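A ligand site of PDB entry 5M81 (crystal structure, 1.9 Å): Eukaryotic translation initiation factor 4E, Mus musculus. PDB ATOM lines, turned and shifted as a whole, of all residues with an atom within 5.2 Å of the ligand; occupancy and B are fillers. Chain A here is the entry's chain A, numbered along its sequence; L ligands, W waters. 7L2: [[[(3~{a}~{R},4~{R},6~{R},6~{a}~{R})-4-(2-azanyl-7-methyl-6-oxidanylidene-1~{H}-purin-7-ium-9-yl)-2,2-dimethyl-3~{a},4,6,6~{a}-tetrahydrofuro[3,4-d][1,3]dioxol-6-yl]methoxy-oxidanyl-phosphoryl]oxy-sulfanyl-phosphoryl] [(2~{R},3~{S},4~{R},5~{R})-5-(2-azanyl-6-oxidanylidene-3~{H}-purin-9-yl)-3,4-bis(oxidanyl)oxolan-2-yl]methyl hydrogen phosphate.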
ATOM      1  N   PHE A  21     -16.982  -9.096 -19.909  1.00  0.00           N
ATOM      2  CA  PHE A  21     -15.730  -8.972 -19.194  1.00  0.00           C
ATOM      3  C   PHE A  21     -16.040  -8.994 -17.716  1.00  0.00           C
ATOM      4  O   PHE A  21     -16.964  -8.317 -17.261  1.00  0.00           O
ATOM      5  CB  PHE A  21     -15.008  -7.671 -19.564  1.00  0.00           C
ATOM      6  CG  PHE A  21     -13.817  -7.365 -18.684  1.00  0.00           C
ATOM      7  CD1 PHE A  21     -12.531  -7.714 -19.104  1.00  0.00           C
ATOM      8  CD2 PHE A  21     -13.966  -6.711 -17.466  1.00  0.00           C
ATOM      9  CE1 PHE A  21     -11.436  -7.420 -18.311  1.00  0.00           C
ATOM     10  CE2 PHE A  21     -12.877  -6.438 -16.675  1.00  0.00           C
ATOM     11  CZ  PHE A  21     -11.613  -6.796 -17.090  1.00  0.00           C
ATOM     12  N   ASN A  23     -14.006  -8.672 -14.001  1.00  0.00           N
ATOM     13  CA  ASN A  23     -12.736  -8.395 -13.348  1.00  0.00           C
ATOM     14  C   ASN A  23     -12.291  -9.626 -12.565  1.00  0.00           C
ATOM     15  O   ASN A  23     -13.041 -10.191 -11.762  1.00  0.00           O
ATOM     16  CB  ASN A  23     -12.847  -7.178 -12.427  1.00  0.00           C
ATOM     17  CG  ASN A  23     -11.499  -6.656 -12.029  1.00  0.00           C
ATOM     18  OD1 ASN A  23     -10.790  -7.277 -11.250  1.00  0.00           O
ATOM     19  ND2 ASN A  23     -11.120  -5.507 -12.585  1.00  0.00           N
ATOM     20  N   ASP A  24     -11.060 -10.039 -12.818  1.00  0.00           N
ATOM     21  CA  ASP A  24     -10.409 -11.049 -11.996  1.00  0.00           C
ATOM     22  C   ASP A  24      -8.937 -10.650 -11.975  1.00  0.00           C
ATOM     23  O   ASP A  24      -8.274 -10.704 -13.011  1.00  0.00           O
ATOM     24  CB  ASP A  24     -10.611 -12.463 -12.548  1.00  0.00           C
ATOM     25  CG  ASP A  24      -9.999 -13.554 -11.669  1.00  0.00           C
ATOM     26  OD1 ASP A  24     -10.309 -14.747 -11.897  1.00  0.00           O
ATOM     27  OD2 ASP A  24      -9.194 -13.228 -10.769  1.00  0.00           O
ATOM     28  N   LYS A  25      -8.449 -10.210 -10.814  1.00  0.00           N
ATOM     29  CA  LYS A  25      -7.074  -9.765 -10.719  1.00  0.00           C
ATOM     30  C   LYS A  25      -6.065 -10.899 -10.875  1.00  0.00           C
ATOM     31  O   LYS A  25      -4.861 -10.611 -10.947  1.00  0.00           O
ATOM     32  CB  LYS A  25      -6.841  -9.064  -9.382  1.00  0.00           C
ATOM     33  CG  LYS A  25      -7.485  -7.691  -9.239  1.00  0.00           C
ATOM     34  CD  LYS A  25      -7.084  -7.158  -7.859  1.00  0.00           C
ATOM     35  CE  LYS A  25      -7.906  -5.998  -7.405  1.00  0.00           C
ATOM     36  NZ  LYS A  25      -7.576  -5.734  -5.973  1.00  0.00           N
ATOM     37  N   SER A  26      -6.521 -12.160 -10.893  1.00  0.00           N
ATOM     38  CA  SER A  26      -5.660 -13.304 -11.204  1.00  0.00           C
ATOM     39  C   SER A  26      -5.212 -13.325 -12.657  1.00  0.00           C
ATOM     40  O   SER A  26      -4.251 -14.049 -12.982  1.00  0.00           O
ATOM     41  CB  SER A  26      -6.414 -14.616 -10.950  1.00  0.00           C
ATOM     42  OG  SER A  26      -6.555 -14.874  -9.581  1.00  0.00           O
ATOM     43  N   LYS A  27      -5.904 -12.620 -13.531  1.00  0.00           N
ATOM     44  CA  LYS A  27      -5.764 -12.784 -14.974  1.00  0.00           C
ATOM     45  C   LYS A  27      -5.426 -11.457 -15.641  1.00  0.00           C
ATOM     46  O   LYS A  27      -5.676 -10.381 -15.101  1.00  0.00           O
ATOM     47  CB  LYS A  27      -7.063 -13.357 -15.574  1.00  0.00           C
ATOM     48  CG  LYS A  27      -7.444 -14.710 -14.968  1.00  0.00           C
ATOM     49  CD  LYS A  27      -8.954 -14.977 -15.041  1.00  0.00           C
ATOM     50  CE  LYS A  27      -9.423 -15.247 -16.456  1.00  0.00           C
ATOM     51  NZ  LYS A  27     -10.879 -15.566 -16.506  1.00  0.00           N
ATOM     52  N   THR A  28      -4.848 -11.552 -16.842  1.00  0.00           N
ATOM     53  CA  THR A  28      -4.661 -10.360 -17.639  1.00  0.00           C
ATOM     54  C   THR A  28      -6.019  -9.829 -18.082  1.00  0.00           C
ATOM     55  O   THR A  28      -7.018 -10.554 -18.064  1.00  0.00           O
ATOM     56  CB  THR A  28      -3.809 -10.627 -18.879  1.00  0.00           C
ATOM     57  OG1 THR A  28      -4.485 -11.607 -19.697  1.00  0.00           O
ATOM     58  CG2 THR A  28      -2.417 -11.135 -18.497  1.00  0.00           C
ATOM     59  N   TRP A  29      -6.019  -8.578 -18.523  1.00  0.00           N
ATOM     60  CA  TRP A  29      -7.258  -7.964 -19.004  1.00  0.00           C
ATOM     61  C   TRP A  29      -7.785  -8.703 -20.233  1.00  0.00           C
ATOM     62  O   TRP A  29      -8.972  -9.010 -20.323  1.00  0.00           O
ATOM     63  CB  TRP A  29      -7.008  -6.483 -19.320  1.00  0.00           C
ATOM     64  CG  TRP A  29      -8.239  -5.801 -19.762  1.00  0.00           C
ATOM     65  CD1 TRP A  29      -9.193  -5.210 -18.982  1.00  0.00           C
ATOM     66  CD2 TRP A  29      -8.686  -5.667 -21.120  1.00  0.00           C
ATOM     67  NE1 TRP A  29     -10.210  -4.700 -19.770  1.00  0.00           N
ATOM     68  CE2 TRP A  29      -9.920  -4.972 -21.087  1.00  0.00           C
ATOM     69  CE3 TRP A  29      -8.161  -6.052 -22.350  1.00  0.00           C
ATOM     70  CZ2 TRP A  29     -10.629  -4.667 -22.254  1.00  0.00           C
ATOM     71  CZ3 TRP A  29      -8.866  -5.745 -23.504  1.00  0.00           C
ATOM     72  CH2 TRP A  29     -10.088  -5.063 -23.443  1.00  0.00           C
ATOM     73  N   GLN A  30      -6.898  -9.018 -21.174  1.00  0.00           N
ATOM     74  CA  GLN A  30      -7.327  -9.759 -22.359  1.00  0.00           C
ATOM     75  C   GLN A  30      -7.919 -11.113 -21.975  1.00  0.00           C
ATOM     76  O   GLN A  30      -8.912 -11.544 -22.546  1.00  0.00           O
ATOM     77  CB  GLN A  30      -6.136  -9.927 -23.302  1.00  0.00           C
ATOM     78  CG  GLN A  30      -5.508  -8.600 -23.793  1.00  0.00           C
ATOM     79  CD  GLN A  30      -4.497  -7.970 -22.813  1.00  0.00           C
ATOM     80  OE1 GLN A  30      -4.293  -8.442 -21.691  1.00  0.00           O
ATOM     81  NE2 GLN A  30      -3.855  -6.898 -23.266  1.00  0.00           N
ATOM     82  N   ASN A  32      -9.594 -11.889 -19.367  1.00  0.00           N
ATOM     83  CA  ASN A  32     -10.896 -11.698 -18.724  1.00  0.00           C
ATOM     84  C   ASN A  32     -12.011 -11.374 -19.699  1.00  0.00           C
ATOM     85  O   ASN A  32     -13.186 -11.304 -19.288  1.00  0.00           O
ATOM     86  CB  ASN A  32     -10.762 -10.572 -17.700  1.00  0.00           C
ATOM     87  CG  ASN A  32     -10.189 -11.075 -16.416  1.00  0.00           C
ATOM     88  OD1 ASN A  32     -10.448 -12.215 -16.034  1.00  0.00           O
ATOM     89  ND2 ASN A  32      -9.310 -10.290 -15.794  1.00  0.00           N
ATOM     90  N   PRO A  73     -13.176  -5.975 -28.959  1.00  0.00           N
ATOM     91  CA  PRO A  73     -13.449  -4.714 -28.248  1.00  0.00           C
ATOM     92  C   PRO A  73     -12.256  -4.242 -27.421  1.00  0.00           C
ATOM     93  O   PRO A  73     -12.333  -4.069 -26.198  1.00  0.00           O
ATOM     94  CB  PRO A  73     -14.651  -5.083 -27.377  1.00  0.00           C
ATOM     95  CG  PRO A  73     -14.379  -6.539 -27.007  1.00  0.00           C
ATOM     96  CD  PRO A  73     -13.817  -7.137 -28.304  1.00  0.00           C
ATOM     97  N   MET A  74     -11.139  -3.997 -28.103  1.00  0.00           N
ATOM     98  CA  MET A  74      -9.888  -3.634 -27.449  1.00  0.00           C
ATOM     99  C   MET A  74      -9.120  -2.661 -28.319  1.00  0.00           C
ATOM    100  O   MET A  74      -9.234  -2.668 -29.558  1.00  0.00           O
ATOM    101  CB  MET A  74      -9.100  -4.915 -27.111  1.00  0.00           C
ATOM    102  CG  MET A  74      -8.718  -5.775 -28.317  1.00  0.00           C
ATOM    103  SD  MET A  74      -7.572  -7.081 -27.867  1.00  0.00           S
ATOM    104  CE  MET A  74      -8.729  -8.204 -27.108  1.00  0.00           C
ATOM    105  N   TRP A  75      -8.361  -1.784 -27.638  1.00  0.00           N
ATOM    106  CA  TRP A  75      -7.593  -0.753 -28.347  1.00  0.00           C
ATOM    107  C   TRP A  75      -6.689  -1.364 -29.392  1.00  0.00           C
ATOM    108  O   TRP A  75      -6.435  -0.741 -30.419  1.00  0.00           O
ATOM    109  CB  TRP A  75      -6.719   0.063 -27.406  1.00  0.00           C
ATOM    110  CG  TRP A  75      -7.374   0.662 -26.226  1.00  0.00           C
ATOM    111  CD1 TRP A  75      -8.615   1.250 -26.155  1.00  0.00           C
ATOM    112  CD2 TRP A  75      -6.832   0.719 -24.924  1.00  0.00           C
ATOM    113  NE1 TRP A  75      -8.860   1.682 -24.864  1.00  0.00           N
ATOM    114  CE2 TRP A  75      -7.780   1.359 -24.092  1.00  0.00           C
ATOM    115  CE3 TRP A  75      -5.629   0.280 -24.377  1.00  0.00           C
ATOM    116  CZ2 TRP A  75      -7.550   1.573 -22.762  1.00  0.00           C
ATOM    117  CZ3 TRP A  75      -5.406   0.497 -23.053  1.00  0.00           C
ATOM    118  CH2 TRP A  75      -6.361   1.133 -22.249  1.00  0.00           C
ATOM    119  N   GLU A  76      -6.166  -2.568 -29.120  1.00  0.00           N
ATOM    120  CA  GLU A  76      -5.172  -3.197 -29.985  1.00  0.00           C
ATOM    121  C   GLU A  76      -5.732  -3.588 -31.348  1.00  0.00           C
ATOM    122  O   GLU A  76      -4.954  -3.814 -32.263  1.00  0.00           O
ATOM    123  CB  GLU A  76      -4.586  -4.459 -29.340  1.00  0.00           C
ATOM    124  CG  GLU A  76      -3.654  -4.261 -28.131  1.00  0.00           C
ATOM    125  CD  GLU A  76      -4.353  -3.783 -26.874  1.00  0.00           C
ATOM    126  OE1 GLU A  76      -5.603  -3.705 -26.863  1.00  0.00           O
ATOM    127  OE2 GLU A  76      -3.642  -3.515 -25.872  1.00  0.00           O
ATOM    128  N   ASN A 128     -19.178   0.049 -18.902  1.00  0.00           N
ATOM    129  CA  ASN A 128     -18.401  -0.347 -17.730  1.00  0.00           C
ATOM    130  C   ASN A 128     -19.284  -0.149 -16.503  1.00  0.00           C
ATOM    131  O   ASN A 128     -19.723   0.969 -16.240  1.00  0.00           O
ATOM    132  CB  ASN A 128     -17.142   0.514 -17.584  1.00  0.00           C
ATOM    133  CG  ASN A 128     -16.337   0.619 -18.864  1.00  0.00           C
ATOM    134  OD1 ASN A 128     -16.262   1.686 -19.487  1.00  0.00           O
ATOM    135  ND2 ASN A 128     -15.692  -0.464 -19.230  1.00  0.00           N
ATOM    136  N   ARG A 130     -19.122   0.042 -12.667  1.00  0.00           N
ATOM    137  CA  ARG A 130     -18.063   0.299 -11.699  1.00  0.00           C
ATOM    138  C   ARG A 130     -18.632   0.972 -10.454  1.00  0.00           C
ATOM    139  O   ARG A 130     -19.531   1.802 -10.567  1.00  0.00           O
ATOM    140  CB  ARG A 130     -16.954   1.198 -12.278  1.00  0.00           C
ATOM    141  CG  ARG A 130     -16.257   0.639 -13.524  1.00  0.00           C
ATOM    142  CD  ARG A 130     -15.315  -0.503 -13.122  1.00  0.00           C
ATOM    143  NE  ARG A 130     -14.507  -0.945 -14.263  1.00  0.00           N
ATOM    144  CZ  ARG A 130     -14.974  -1.707 -15.260  1.00  0.00           C
ATOM    145  NH1 ARG A 130     -16.238  -2.126 -15.230  1.00  0.00           N
ATOM    146  NH2 ARG A 130     -14.168  -2.050 -16.267  1.00  0.00           N
ATOM    147  N   LYS A 132     -17.269   3.182  -8.642  1.00  0.00           N
ATOM    148  CA  LYS A 132     -16.983   4.606  -8.601  1.00  0.00           C
ATOM    149  C   LYS A 132     -17.815   5.405  -9.588  1.00  0.00           C
ATOM    150  O   LYS A 132     -17.772   6.638  -9.560  1.00  0.00           O
ATOM    151  CB  LYS A 132     -15.489   4.878  -8.853  1.00  0.00           C
ATOM    152  CG  LYS A 132     -15.002   4.562 -10.267  1.00  0.00           C
ATOM    153  CD  LYS A 132     -13.638   5.217 -10.534  1.00  0.00           C
ATOM    154  CE  LYS A 132     -12.797   4.444 -11.564  1.00  0.00           C
ATOM    155  NZ  LYS A 132     -13.609   3.869 -12.677  1.00  0.00           N
ATOM    156  N   LYS A 135     -19.873   3.878 -16.966  1.00  0.00           N
ATOM    157  CA  LYS A 135     -19.520   4.563 -18.200  1.00  0.00           C
ATOM    158  C   LYS A 135     -20.119   3.809 -19.381  1.00  0.00           C
ATOM    159  O   LYS A 135     -20.138   2.569 -19.376  1.00  0.00           O
ATOM    160  CB  LYS A 135     -18.000   4.663 -18.354  1.00  0.00           C
ATOM    161  CG  LYS A 135     -17.337   5.579 -17.320  1.00  0.00           C
ATOM    162  CD  LYS A 135     -15.846   5.670 -17.525  1.00  0.00           C
ATOM    163  CE  LYS A 135     -15.127   4.533 -16.832  1.00  0.00           C
ATOM    164  NZ  LYS A 135     -13.662   4.783 -16.878  1.00  0.00           N
ATOM    165  N   TRP A 139     -17.410   3.533 -29.666  1.00  0.00           N
ATOM    166  CA  TRP A 139     -16.056   3.499 -30.196  1.00  0.00           C
ATOM    167  C   TRP A 139     -16.107   3.692 -31.710  1.00  0.00           C
ATOM    168  O   TRP A 139     -16.899   3.020 -32.382  1.00  0.00           O
ATOM    169  CB  TRP A 139     -15.387   2.163 -29.889  1.00  0.00           C
ATOM    170  CG  TRP A 139     -14.982   1.965 -28.462  1.00  0.00           C
ATOM    171  CD1 TRP A 139     -15.562   2.510 -27.351  1.00  0.00           C
ATOM    172  CD2 TRP A 139     -13.893   1.159 -28.008  1.00  0.00           C
ATOM    173  NE1 TRP A 139     -14.876   2.089 -26.213  1.00  0.00           N
ATOM    174  CE2 TRP A 139     -13.856   1.248 -26.602  1.00  0.00           C
ATOM    175  CE3 TRP A 139     -12.935   0.369 -28.660  1.00  0.00           C
ATOM    176  CZ2 TRP A 139     -12.887   0.582 -25.832  1.00  0.00           C
ATOM    177  CZ3 TRP A 139     -11.981  -0.292 -27.902  1.00  0.00           C
ATOM    178  CH2 TRP A 139     -11.962  -0.178 -26.495  1.00  0.00           C
ATOM    179  N   THR A 176      -5.950   7.395 -24.201  1.00  0.00           N
ATOM    180  CA  THR A 176      -6.448   6.603 -23.073  1.00  0.00           C
ATOM    181  C   THR A 176      -5.455   5.546 -22.644  1.00  0.00           C
ATOM    182  O   THR A 176      -5.292   5.290 -21.447  1.00  0.00           O
ATOM    183  CB  THR A 176      -7.772   5.936 -23.457  1.00  0.00           C
ATOM    184  OG1 THR A 176      -8.692   6.922 -23.930  1.00  0.00           O
ATOM    185  CG2 THR A 176      -8.386   5.214 -22.254  1.00  0.00           C
ATOM    186  N   LYS A 179      -1.215   6.853 -20.193  1.00  0.00           N
ATOM    187  CA  LYS A 179      -1.833   7.647 -19.144  1.00  0.00           C
ATOM    188  C   LYS A 179      -1.509   7.085 -17.766  1.00  0.00           C
ATOM    189  O   LYS A 179      -2.003   6.019 -17.392  1.00  0.00           O
ATOM    190  CB  LYS A 179      -3.346   7.696 -19.355  1.00  0.00           C
ATOM    191  CG  LYS A 179      -4.149   8.357 -18.246  1.00  0.00           C
ATOM    192  CD  LYS A 179      -5.624   7.941 -18.336  1.00  0.00           C
ATOM    193  CE  LYS A 179      -5.777   6.428 -18.221  1.00  0.00           C
ATOM    194  NZ  LYS A 179      -7.163   6.017 -17.872  1.00  0.00           N
ATOM    195  N   SER A 182      -5.219   9.085 -14.590  1.00  0.00           N
ATOM    196  CA  SER A 182      -6.615   8.819 -14.273  1.00  0.00           C
ATOM    197  C   SER A 182      -7.563   9.185 -15.416  1.00  0.00           C
ATOM    198  O   SER A 182      -8.436   8.394 -15.783  1.00  0.00           O
ATOM    199  CB  SER A 182      -7.041   9.575 -13.013  1.00  0.00           C
HETATM  200  O1  7L2 L   1      -8.582  -7.513 -16.219  1.00  0.00           O
HETATM  201  C1  7L2 L   1      -7.852  -7.061 -15.298  1.00  0.00           C
HETATM  202  N1  7L2 L   1      -6.880  -7.824 -14.779  1.00  0.00           N
HETATM  203  C2  7L2 L   1      -6.094  -7.378 -13.796  1.00  0.00           C
HETATM  204  N2  7L2 L   1      -5.117  -8.184 -13.288  1.00  0.00           N
HETATM  205  N3  7L2 L   1      -6.255  -6.125 -13.293  1.00  0.00           N
HETATM  206  C3  7L2 L   1      -7.227  -5.312 -13.804  1.00  0.00           C
HETATM  207  C4  7L2 L   1      -8.056  -5.764 -14.820  1.00  0.00           C
HETATM  208  N4  7L2 L   1      -8.920  -4.742 -15.128  1.00  0.00           N
HETATM  209  C5  7L2 L   1      -8.623  -3.715 -14.304  1.00  0.00           C
HETATM  210  N5  7L2 L   1      -7.592  -4.063 -13.518  1.00  0.00           N
HETATM  211  C6  7L2 L   1      -6.965  -3.247 -12.440  1.00  0.00           C
HETATM  212  O2  7L2 L   1      -7.988  -2.436 -11.863  1.00  0.00           O
HETATM  213  C7  7L2 L   1      -5.930  -2.300 -12.972  1.00  0.00           C
HETATM  214  O3  7L2 L   1      -5.000  -2.128 -11.905  1.00  0.00           O
HETATM  215  C8  7L2 L   1      -6.718  -1.034 -13.235  1.00  0.00           C
HETATM  216  O4  7L2 L   1      -5.897   0.144 -13.208  1.00  0.00           O
HETATM  217  C9  7L2 L   1      -7.727  -1.053 -12.111  1.00  0.00           C
HETATM  218  C10 7L2 L   1      -9.024  -0.345 -12.475  1.00  0.00           C
HETATM  219  O5  7L2 L   1      -9.504  -0.830 -13.733  1.00  0.00           O
HETATM  220  P1  7L2 L   1     -10.906  -0.253 -14.283  1.00  0.00           P
HETATM  221  O6  7L2 L   1     -11.811  -0.314 -13.074  1.00  0.00           O
HETATM  222  O7  7L2 L   1     -11.251  -0.990 -15.568  1.00  0.00           O
HETATM  223  O8  7L2 L   1     -10.472   1.256 -14.645  1.00  0.00           O
HETATM  224  P2  7L2 L   1     -11.283   2.303 -15.568  1.00  0.00           P
HETATM  225  O9  7L2 L   1     -11.287   3.609 -14.866  1.00  0.00           O
HETATM  226  S1  7L2 L   1     -13.184   1.652 -15.984  1.00  0.00           S
HETATM  227  O10 7L2 L   1     -10.485   2.437 -16.975  1.00  0.00           O
HETATM  228  P3  7L2 L   1      -8.920   2.839 -17.166  1.00  0.00           P
HETATM  229  O11 7L2 L   1      -8.400   3.702 -16.033  1.00  0.00           O
HETATM  230  O12 7L2 L   1      -8.781   3.286 -18.604  1.00  0.00           O
HETATM  231  O13 7L2 L   1      -8.181   1.423 -17.032  1.00  0.00           O
HETATM  232  C11 7L2 L   1      -8.558   0.349 -17.898  1.00  0.00           C
HETATM  233  C12 7L2 L   1      -7.994  -0.923 -17.297  1.00  0.00           C
HETATM  234  O14 7L2 L   1      -8.437  -2.008 -18.088  1.00  0.00           O
HETATM  235  C13 7L2 L   1      -6.481  -0.944 -17.419  1.00  0.00           C
HETATM  236  O15 7L2 L   1      -6.002  -1.887 -16.486  1.00  0.00           O
HETATM  237  C14 7L2 L   1      -4.934  -2.612 -17.091  1.00  0.00           C
HETATM  238  C15 7L2 L   1      -4.994  -4.067 -16.646  1.00  0.00           C
HETATM  239  C16 7L2 L   1      -3.631  -1.958 -16.672  1.00  0.00           C
HETATM  240  O16 7L2 L   1      -5.116  -2.493 -18.514  1.00  0.00           O
HETATM  241  C17 7L2 L   1      -6.160  -1.559 -18.762  1.00  0.00           C
HETATM  242  C18 7L2 L   1      -7.429  -2.338 -19.070  1.00  0.00           C
HETATM  243  N6  7L2 L   1      -7.978  -2.089 -20.427  1.00  0.00           N
HETATM  244  C19 7L2 L   1      -9.175  -1.550 -20.733  1.00  0.00           C
HETATM  245  N7  7L2 L   1      -9.318  -1.567 -22.073  1.00  0.00           N
HETATM  246  C20 7L2 L   1     -10.489  -1.030 -22.809  1.00  0.00           C
HETATM  247  C21 7L2 L   1      -8.203  -2.126 -22.588  1.00  0.00           C
HETATM  248  C22 7L2 L   1      -7.370  -2.461 -21.554  1.00  0.00           C
HETATM  249  N8  7L2 L   1      -6.181  -3.066 -21.801  1.00  0.00           N
HETATM  250  C23 7L2 L   1      -5.793  -3.340 -23.073  1.00  0.00           C
HETATM  251  N9  7L2 L   1      -4.586  -3.941 -23.273  1.00  0.00           N
HETATM  252  N10 7L2 L   1      -6.609  -3.016 -24.117  1.00  0.00           N
HETATM  253  C24 7L2 L   1      -7.815  -2.415 -23.917  1.00  0.00           C
HETATM  254  O17 7L2 L   1      -8.589  -2.120 -25.009  1.00  0.00           O
HETATM  255  O   HOH W   1     -12.220  -2.617 -12.142  1.00  0.00           O
HETATM  256  O   HOH W   2      -8.850   3.552 -12.809  1.00  0.00           O
HETATM  257  O   HOH W   3     -12.730   1.259 -11.403  1.00  0.00           O
HETATM  258  O   HOH W   4      -6.355   3.119 -19.484  1.00  0.00           O
HETATM  259  O   HOH W   5      -3.654  -8.233 -10.798  1.00  0.00           O
HETATM  260  O   HOH W   6      -2.535  -0.032 -13.349  1.00  0.00           O
HETATM  261  O   HOH W   7     -11.287   5.121 -18.985  1.00  0.00           O
HETATM  262  O   HOH W   8      -3.757  -4.866 -20.177  1.00  0.00           O
HETATM  263  O   HOH W   9     -13.563  -2.099 -22.031  1.00  0.00           O
HETATM  264  O   HOH W  10     -11.189  -3.506 -16.111  1.00  0.00           O
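Water W3 lies within hydrogen-bond range of an oxygen (O6) of the ligand (2.5 Å) and the side-chain amino group (NZ) of Lys 132 (3.0 Å). Water W1 lies within hydrogen-bond range of O6 of the ligand (2.5 Å) and ND2 of Asn 23 (3.1 Å). Water W10 lies within hydrogen-bond range of an oxygen (O7) of the ligand (2.6 Å) and the guanidinium group (NH2) of Arg 130 (3.3 Å). Water W4 lies within hydrogen-bond range of O12 of the ligand, O of Thr 176 and NZ of Lys 179. Water W5 bridges the backbone carbonyl oxygen (O) of Lys 25 (2.7 Å) and a nitrogen (N2) of the ligand (2.9 Å). Water W7 bridges an oxygen (O12) of the ligand (3.1 Å) and the side-chain amino group (NZ) of Lys 135 (3.2 Å).
NE1 of Trp 29 sits close to N6 of the ligand (3.5 Å). Phe 21 touches the ligand (CZ to O1, 3.2 Å). O of Asp 24 touches N1 of the ligand (3.7 Å). Thr 28 touches the ligand. Met 74 touches the ligand. Hydrophobic or aromatic side chains within 4 Å of the ligand: Phe 21, Trp 29, Met 74 and Trp 75. Within 4 Å of the ligand: Phe 21, Asn 23, Asp 24, Lys 25, Lys 27, Thr 28, Trp 29, Gln 30, Asn 32, Met 74, Trp 75, Glu 76, Arg 130, Lys 132, Lys 135 and Lys 179. The nearest printed residue that does not touch the ligand is Trp 139 (4.1 Å).
The backbone carbonyl oxygen of Lys 135 sits at hydrogen-bond distance from the backbone NH of Asn 128 (2.7 Å). ND2 of Asn 32 lies within hydrogen-bond range of O of Asp 24, 3.0 Å away. The side-chain amide nitrogen of Asn 32 sits at hydrogen-bond distance from the backbone carbonyl oxygen of Thr 28. The side-chain amino group (NZ) of Lys 27 lies close to the side-chain amide oxygen (OD1) of Asn 32, 3.4 Å away. The side-chain amino group (NZ) of Lys 179 lies within hydrogen-bond range of the backbone carbonyl oxygen (O) of Ser 182 (3.4 Å). The backbone NH (N) of Ser 26 lies within hydrogen-bond range of the side-chain carboxylate (OD2) of Asp 24 (2.9 Å).
A nitrogen (N9) of the ligand lies close to the side-chain amide nitrogen of Gln 30 (3.0 Å). The side-chain amide nitrogen (ND2) of Asn 23 lies within hydrogen-bond range of a nitrogen (N4) of the ligand (3.4 Å). The backbone carbonyl oxygen (O) of Lys 27 is in hydrogen-bond range of a nitrogen (N2) of the ligand, at 2.9 Å. S1 of the ligand lies close to NZ of Lys 135 (3.3 Å). A nitrogen (N2) of the ligand is in hydrogen-bond range of the backbone carbonyl oxygen (O) of Lys 25 (3.4 Å). The side-chain carboxylate of Glu 76 is in hydrogen-bond range of a nitrogen (N9) of the ligand (2.8 Å). The side-chain amino group (NZ) of Lys 132 lies within hydrogen-bond range of an oxygen (O9) of the ligand. O6 of the ligand is in salt-bridge range of NE of Arg 130 (3.0 Å). The backbone NH (N) of Trp 75 sits at hydrogen-bond distance from an oxygen (O17) of the ligand. The side-chain amide nitrogen of Asn 32 lies within hydrogen-bond range of an oxygen (O1) of the ligand (2.9 Å). An oxygen (O11) of the ligand lies within salt-bridge range of the side-chain amino group (NZ) of Lys 179.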
